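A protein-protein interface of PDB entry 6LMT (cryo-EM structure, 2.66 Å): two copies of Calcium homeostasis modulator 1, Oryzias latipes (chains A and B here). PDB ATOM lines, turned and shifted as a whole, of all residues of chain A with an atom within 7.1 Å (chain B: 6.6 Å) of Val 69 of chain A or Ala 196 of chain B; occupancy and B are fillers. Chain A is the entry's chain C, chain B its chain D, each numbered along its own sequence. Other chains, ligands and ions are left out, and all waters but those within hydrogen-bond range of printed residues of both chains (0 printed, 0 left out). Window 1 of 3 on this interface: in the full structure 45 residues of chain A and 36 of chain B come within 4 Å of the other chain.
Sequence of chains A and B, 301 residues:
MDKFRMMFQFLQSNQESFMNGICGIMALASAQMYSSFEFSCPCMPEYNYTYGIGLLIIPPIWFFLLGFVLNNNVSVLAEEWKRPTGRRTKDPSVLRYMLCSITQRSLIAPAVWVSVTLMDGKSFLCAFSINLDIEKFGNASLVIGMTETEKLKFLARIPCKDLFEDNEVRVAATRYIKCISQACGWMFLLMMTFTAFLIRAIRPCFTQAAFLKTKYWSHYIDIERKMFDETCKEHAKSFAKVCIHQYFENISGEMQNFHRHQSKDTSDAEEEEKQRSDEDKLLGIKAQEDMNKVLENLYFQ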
ATOM      1  N   PHE A  64      -8.815  22.098  28.820  1.00  0.00           N
ATOM      2  CA  PHE A  64      -8.302  20.745  28.679  1.00  0.00           C
ATOM      3  C   PHE A  64      -8.993  20.003  27.543  1.00  0.00           C
ATOM      4  O   PHE A  64      -8.336  19.340  26.734  1.00  0.00           O
ATOM      5  CB  PHE A  64      -8.474  20.016  30.003  1.00  0.00           C
ATOM      6  CG  PHE A  64      -7.963  18.627  30.004  1.00  0.00           C
ATOM      7  CD1 PHE A  64      -6.612  18.379  29.929  1.00  0.00           C
ATOM      8  CD2 PHE A  64      -8.826  17.564  30.135  1.00  0.00           C
ATOM      9  CE1 PHE A  64      -6.134  17.098  29.945  1.00  0.00           C
ATOM     10  CE2 PHE A  64      -8.346  16.279  30.160  1.00  0.00           C
ATOM     11  CZ  PHE A  64      -6.997  16.051  30.065  1.00  0.00           C
ATOM     12  N   LEU A  65     -10.324  20.106  27.467  1.00  0.00           N
ATOM     13  CA  LEU A  65     -11.070  19.492  26.374  1.00  0.00           C
ATOM     14  C   LEU A  65     -10.739  20.130  25.043  1.00  0.00           C
ATOM     15  O   LEU A  65     -10.752  19.464  24.009  1.00  0.00           O
ATOM     16  CB  LEU A  65     -12.564  19.615  26.613  1.00  0.00           C
ATOM     17  CG  LEU A  65     -13.243  18.806  27.685  1.00  0.00           C
ATOM     18  CD1 LEU A  65     -14.663  19.277  27.740  1.00  0.00           C
ATOM     19  CD2 LEU A  65     -13.175  17.360  27.300  1.00  0.00           C
ATOM     20  N   LEU A  66     -10.473  21.427  25.050  1.00  0.00           N
ATOM     21  CA  LEU A  66     -10.112  22.131  23.835  1.00  0.00           C
ATOM     22  C   LEU A  66      -8.753  21.691  23.319  1.00  0.00           C
ATOM     23  O   LEU A  66      -8.499  21.761  22.118  1.00  0.00           O
ATOM     24  CB  LEU A  66     -10.137  23.626  24.109  1.00  0.00           C
ATOM     25  CG  LEU A  66     -10.015  24.598  22.965  1.00  0.00           C
ATOM     26  CD1 LEU A  66     -11.191  24.402  22.084  1.00  0.00           C
ATOM     27  CD2 LEU A  66      -9.989  25.981  23.513  1.00  0.00           C
ATOM     28  N   GLY A  67      -7.874  21.228  24.201  1.00  0.00           N
ATOM     29  CA  GLY A  67      -6.638  20.631  23.747  1.00  0.00           C
ATOM     30  C   GLY A  67      -6.835  19.297  23.062  1.00  0.00           C
ATOM     31  O   GLY A  67      -6.078  18.948  22.159  1.00  0.00           O
ATOM     32  N   PHE A  68      -7.828  18.526  23.491  1.00  0.00           N
ATOM     33  CA  PHE A  68      -8.162  17.286  22.798  1.00  0.00           C
ATOM     34  C   PHE A  68      -8.871  17.522  21.475  1.00  0.00           C
ATOM     35  O   PHE A  68      -8.694  16.745  20.542  1.00  0.00           O
ATOM     36  CB  PHE A  68      -9.044  16.414  23.676  1.00  0.00           C
ATOM     37  CG  PHE A  68      -8.326  15.754  24.788  1.00  0.00           C
ATOM     38  CD1 PHE A  68      -6.989  15.489  24.704  1.00  0.00           C
ATOM     39  CD2 PHE A  68      -8.988  15.427  25.943  1.00  0.00           C
ATOM     40  CE1 PHE A  68      -6.324  14.877  25.736  1.00  0.00           C
ATOM     41  CE2 PHE A  68      -8.320  14.818  26.979  1.00  0.00           C
ATOM     42  CZ  PHE A  68      -6.983  14.549  26.867  1.00  0.00           C
ATOM     43  N   VAL A  69      -9.694  18.559  21.383  1.00  0.00           N
ATOM     44  CA  VAL A  69     -10.417  18.838  20.150  1.00  0.00           C
ATOM     45  C   VAL A  69      -9.476  19.375  19.081  1.00  0.00           C
ATOM     46  O   VAL A  69      -9.579  19.014  17.908  1.00  0.00           O
ATOM     47  CB  VAL A  69     -11.582  19.800  20.453  1.00  0.00           C
ATOM     48  CG1 VAL A  69     -12.248  20.282  19.204  1.00  0.00           C
ATOM     49  CG2 VAL A  69     -12.596  19.111  21.304  1.00  0.00           C
ATOM     50  N   LEU A  70      -8.522  20.210  19.462  1.00  0.00           N
ATOM     51  CA  LEU A  70      -7.607  20.786  18.490  1.00  0.00           C
ATOM     52  C   LEU A  70      -6.481  19.851  18.084  1.00  0.00           C
ATOM     53  O   LEU A  70      -5.799  20.137  17.099  1.00  0.00           O
ATOM     54  CB  LEU A  70      -7.012  22.084  19.026  1.00  0.00           C
ATOM     55  CG  LEU A  70      -8.009  23.222  19.178  1.00  0.00           C
ATOM     56  CD1 LEU A  70      -7.336  24.429  19.770  1.00  0.00           C
ATOM     57  CD2 LEU A  70      -8.626  23.553  17.853  1.00  0.00           C
ATOM     58  N   ASN A  71      -6.259  18.761  18.804  1.00  0.00           N
ATOM     59  CA  ASN A  71      -5.208  17.820  18.450  1.00  0.00           C
ATOM     60  C   ASN A  71      -5.727  16.869  17.382  1.00  0.00           C
ATOM     61  O   ASN A  71      -6.747  16.206  17.574  1.00  0.00           O
ATOM     62  CB  ASN A  71      -4.757  17.058  19.691  1.00  0.00           C
ATOM     63  CG  ASN A  71      -3.330  16.562  19.603  1.00  0.00           C
ATOM     64  OD1 ASN A  71      -2.691  16.344  20.620  1.00  0.00           O
ATOM     65  ND2 ASN A  71      -2.831  16.356  18.398  1.00  0.00           N
ATOM     66  N   ASN A  72      -5.019  16.792  16.262  1.00  0.00           N
ATOM     67  CA  ASN A  72      -5.466  16.026  15.108  1.00  0.00           C
ATOM     68  C   ASN A  72      -5.067  14.558  15.156  1.00  0.00           C
ATOM     69  O   ASN A  72      -5.224  13.862  14.153  1.00  0.00           O
ATOM     70  CB  ASN A  72      -4.935  16.660  13.824  1.00  0.00           C
ATOM     71  CG  ASN A  72      -5.657  17.931  13.468  1.00  0.00           C
ATOM     72  OD1 ASN A  72      -6.881  17.994  13.519  1.00  0.00           O
ATOM     73  ND2 ASN A  72      -4.906  18.964  13.126  1.00  0.00           N
ATOM     74  N   VAL A  74      -6.228  12.614  17.856  1.00  0.00           N
ATOM     75  CA  VAL A  74      -7.136  11.947  18.776  1.00  0.00           C
ATOM     76  C   VAL A  74      -8.165  11.110  18.040  1.00  0.00           C
ATOM     77  O   VAL A  74      -8.733  10.190  18.632  1.00  0.00           O
ATOM     78  CB  VAL A  74      -7.826  12.959  19.699  1.00  0.00           C
ATOM     79  CG1 VAL A  74      -6.791  13.730  20.476  1.00  0.00           C
ATOM     80  CG2 VAL A  74      -8.705  13.889  18.910  1.00  0.00           C
ATOM     81  N   SER A 106      -2.075  18.967  26.762  1.00  0.00           N
ATOM     82  CA  SER A 106      -3.374  19.574  26.960  1.00  0.00           C
ATOM     83  C   SER A 106      -3.545  20.153  28.347  1.00  0.00           C
ATOM     84  O   SER A 106      -4.593  20.733  28.619  1.00  0.00           O
ATOM     85  CB  SER A 106      -4.471  18.552  26.703  1.00  0.00           C
ATOM     86  OG  SER A 106      -4.453  18.159  25.358  1.00  0.00           O
ATOM     87  N   MET B 191     -20.499  22.428  26.755  1.00  0.00           N
ATOM     88  CA  MET B 191     -21.307  21.486  25.990  1.00  0.00           C
ATOM     89  C   MET B 191     -20.941  21.488  24.516  1.00  0.00           C
ATOM     90  O   MET B 191     -20.996  20.446  23.864  1.00  0.00           O
ATOM     91  CB  MET B 191     -22.788  21.796  26.144  1.00  0.00           C
ATOM     92  CG  MET B 191     -23.351  21.483  27.498  1.00  0.00           C
ATOM     93  SD  MET B 191     -25.135  21.702  27.555  1.00  0.00           S
ATOM     94  CE  MET B 191     -25.277  23.481  27.503  1.00  0.00           C
ATOM     95  N   MET B 192     -20.596  22.641  23.962  1.00  0.00           N
ATOM     96  CA  MET B 192     -20.266  22.664  22.548  1.00  0.00           C
ATOM     97  C   MET B 192     -18.874  22.121  22.287  1.00  0.00           C
ATOM     98  O   MET B 192     -18.618  21.603  21.203  1.00  0.00           O
ATOM     99  CB  MET B 192     -20.385  24.076  21.979  1.00  0.00           C
ATOM    100  CG  MET B 192     -21.775  24.683  22.049  1.00  0.00           C
ATOM    101  SD  MET B 192     -23.153  23.716  21.401  1.00  0.00           S
ATOM    102  CE  MET B 192     -24.038  23.237  22.880  1.00  0.00           C
ATOM    103  N   THR B 193     -17.971  22.218  23.254  1.00  0.00           N
ATOM    104  CA  THR B 193     -16.651  21.637  23.080  1.00  0.00           C
ATOM    105  C   THR B 193     -16.678  20.137  23.316  1.00  0.00           C
ATOM    106  O   THR B 193     -15.930  19.397  22.676  1.00  0.00           O
ATOM    107  CB  THR B 193     -15.659  22.330  24.013  1.00  0.00           C
ATOM    108  OG1 THR B 193     -15.759  23.738  23.815  1.00  0.00           O
ATOM    109  CG2 THR B 193     -14.241  21.943  23.698  1.00  0.00           C
ATOM    110  N   PHE B 194     -17.548  19.666  24.201  1.00  0.00           N
ATOM    111  CA  PHE B 194     -17.681  18.234  24.387  1.00  0.00           C
ATOM    112  C   PHE B 194     -18.426  17.587  23.230  1.00  0.00           C
ATOM    113  O   PHE B 194     -18.167  16.428  22.898  1.00  0.00           O
ATOM    114  CB  PHE B 194     -18.368  17.953  25.713  1.00  0.00           C
ATOM    115  CG  PHE B 194     -18.454  16.514  26.040  1.00  0.00           C
ATOM    116  CD1 PHE B 194     -17.309  15.797  26.333  1.00  0.00           C
ATOM    117  CD2 PHE B 194     -19.674  15.870  26.077  1.00  0.00           C
ATOM    118  CE1 PHE B 194     -17.376  14.462  26.633  1.00  0.00           C
ATOM    119  CE2 PHE B 194     -19.749  14.540  26.387  1.00  0.00           C
ATOM    120  CZ  PHE B 194     -18.600  13.834  26.663  1.00  0.00           C
ATOM    121  N   THR B 195     -19.335  18.324  22.595  1.00  0.00           N
ATOM    122  CA  THR B 195     -19.917  17.878  21.336  1.00  0.00           C
ATOM    123  C   THR B 195     -18.870  17.821  20.236  1.00  0.00           C
ATOM    124  O   THR B 195     -18.850  16.878  19.443  1.00  0.00           O
ATOM    125  CB  THR B 195     -21.059  18.810  20.946  1.00  0.00           C
ATOM    126  OG1 THR B 195     -22.019  18.833  22.000  1.00  0.00           O
ATOM    127  CG2 THR B 195     -21.743  18.342  19.696  1.00  0.00           C
ATOM    128  N   ALA B 196     -17.982  18.812  20.183  1.00  0.00           N
ATOM    129  CA  ALA B 196     -16.891  18.804  19.218  1.00  0.00           C
ATOM    130  C   ALA B 196     -15.920  17.666  19.466  1.00  0.00           C
ATOM    131  O   ALA B 196     -15.305  17.162  18.524  1.00  0.00           O
ATOM    132  CB  ALA B 196     -16.141  20.126  19.269  1.00  0.00           C
ATOM    133  N   PHE B 197     -15.770  17.250  20.718  1.00  0.00           N
ATOM    134  CA  PHE B 197     -14.892  16.134  21.025  1.00  0.00           C
ATOM    135  C   PHE B 197     -15.486  14.815  20.554  1.00  0.00           C
ATOM    136  O   PHE B 197     -14.779  13.985  19.981  1.00  0.00           O
ATOM    137  CB  PHE B 197     -14.604  16.104  22.524  1.00  0.00           C
ATOM    138  CG  PHE B 197     -13.759  14.956  22.943  1.00  0.00           C
ATOM    139  CD1 PHE B 197     -12.424  14.912  22.612  1.00  0.00           C
ATOM    140  CD2 PHE B 197     -14.299  13.913  23.662  1.00  0.00           C
ATOM    141  CE1 PHE B 197     -11.648  13.845  22.985  1.00  0.00           C
ATOM    142  CE2 PHE B 197     -13.523  12.847  24.035  1.00  0.00           C
ATOM    143  CZ  PHE B 197     -12.197  12.817  23.699  1.00  0.00           C
ATOM    144  N   LEU B 198     -16.783  14.610  20.777  1.00  0.00           N
ATOM    145  CA  LEU B 198     -17.425  13.371  20.358  1.00  0.00           C
ATOM    146  C   LEU B 198     -17.557  13.281  18.850  1.00  0.00           C
ATOM    147  O   LEU B 198     -17.535  12.182  18.297  1.00  0.00           O
ATOM    148  CB  LEU B 198     -18.797  13.250  20.998  1.00  0.00           C
ATOM    149  CG  LEU B 198     -18.797  13.034  22.499  1.00  0.00           C
ATOM    150  CD1 LEU B 198     -20.197  13.153  23.041  1.00  0.00           C
ATOM    151  CD2 LEU B 198     -18.234  11.679  22.793  1.00  0.00           C
ATOM    152  N   ILE B 199     -17.704  14.411  18.170  1.00  0.00           N
ATOM    153  CA  ILE B 199     -17.770  14.381  16.717  1.00  0.00           C
ATOM    154  C   ILE B 199     -16.397  14.094  16.123  1.00  0.00           C
ATOM    155  O   ILE B 199     -16.265  13.279  15.212  1.00  0.00           O
ATOM    156  CB  ILE B 199     -18.379  15.692  16.193  1.00  0.00           C
ATOM    157  CG1 ILE B 199     -19.867  15.727  16.510  1.00  0.00           C
ATOM    158  CG2 ILE B 199     -18.173  15.856  14.723  1.00  0.00           C
ATOM    159  CD1 ILE B 199     -20.493  17.057  16.264  1.00  0.00           C
ATOM    160  N   ARG B 200     -15.348  14.705  16.659  1.00  0.00           N
ATOM    161  CA  ARG B 200     -14.014  14.456  16.138  1.00  0.00           C
ATOM    162  C   ARG B 200     -13.370  13.186  16.670  1.00  0.00           C
ATOM    163  O   ARG B 200     -12.201  12.948  16.374  1.00  0.00           O
ATOM    164  CB  ARG B 200     -13.096  15.635  16.427  1.00  0.00           C
ATOM    165  CG  ARG B 200     -13.351  16.830  15.560  1.00  0.00           C
ATOM    166  CD  ARG B 200     -12.405  17.925  15.924  1.00  0.00           C
ATOM    167  NE  ARG B 200     -11.020  17.516  15.735  1.00  0.00           N
ATOM    168  CZ  ARG B 200     -10.341  17.688  14.612  1.00  0.00           C
ATOM    169  NH1 ARG B 200     -10.919  18.265  13.577  1.00  0.00           N
ATOM    170  NH2 ARG B 200      -9.085  17.292  14.529  1.00  0.00           N
ATOM    171  N   ALA B 201     -14.075  12.374  17.444  1.00  0.00           N
ATOM    172  CA  ALA B 201     -13.543  11.090  17.868  1.00  0.00           C
ATOM    173  C   ALA B 201     -14.354   9.909  17.371  1.00  0.00           C
ATOM    174  O   ALA B 201     -13.778   8.896  16.980  1.00  0.00           O
ATOM    175  CB  ALA B 201     -13.455  11.026  19.393  1.00  0.00           C
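OD1 of Asn 72 of chain A is in hydrogen-bond range of NH2 of Arg 200 of chain B (2.5 Å). NE of Arg 200 of chain B sits at hydrogen-bond distance from O of Val 69 of chain A (3.0 Å).
Phe 68 of chain A touches Phe 197 of chain B (CB to CE1, 3.7 Å). Val 69 of chain A touches Thr 193 of chain B (CG2 to O, 3.6 Å). Ala 196 of chain B touches Val 69 of chain A. CG2 of Val 69 of chain A touches N of Phe 197 of chain B, at 3.7 Å. NH2 of Arg 200 of chain B touches O of Asn 71 of chain A (3.99 Å).
Phe 64 of chain A touches none of the printed residues of chain B. Printed residues of chain B within 4 Å of Phe 68 of chain A: Phe 197 (3.7 Å). Val 69 of chain A touches just these residues of chain B: Thr 193 (3.6 Å), Ala 196 (3.9 Å), Phe 197 (3.7 Å) and Arg 200 (3.0 Å). Of the printed residues of chain B, Asn 72 of chain A touches Arg 200. Of the printed residues of chain A, Thr 193 of chain B touches Val 69 (3.6 Å). Ala 196 of chain B touches just one residue of chain A: Val 69 (3.9 Å). Printed residues of chain A within 4 Å of Phe 197 of chain B: Phe 68 (3.7 Å) and Val 69 (3.7 Å). Leu 198 of chain B touches none of the printed residues of chain A. Printed residues of chain A within 4 Å of Arg 200 of chain B: Val 69 (3.0 Å), Asn 71 (3.99 Å) and Asn 72 (2.5 Å). The nearest residue of chain B that does not touch Val 69 of chain A is Phe 194 of chain B (5.8 Å). The nearest printed residue of chain A that does not touch Arg 200 of chain B is Val 74 of chain A (4.4 Å).
Hydrophobic or aromatic side chains of chain A within 4 Å of the printed part of chain B: Phe 68 and Val 69. Along chain A the printed residues that touch a printed residue of chain B span positions 68 to 72. Printed residues of chain B that touch a printed residue of chain A: Thr 193, Ala 196, Phe 197 and Arg 200. Hydrophobic or aromatic side chains of chain B within 4 Å of the printed part of chain A: Ala 196 and Phe 197. Among the printed residues, 7 pairs touch across the chains. Among the printed residues, no Asp or Glu carboxylate lies within 4 Å of a Lys or Arg side-chain nitrogen of the other chain.
No position is printed for both chains. Of the 7 pairs that touch across the chains among the printed residues, none has its exchanged pair printed and touching as well.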
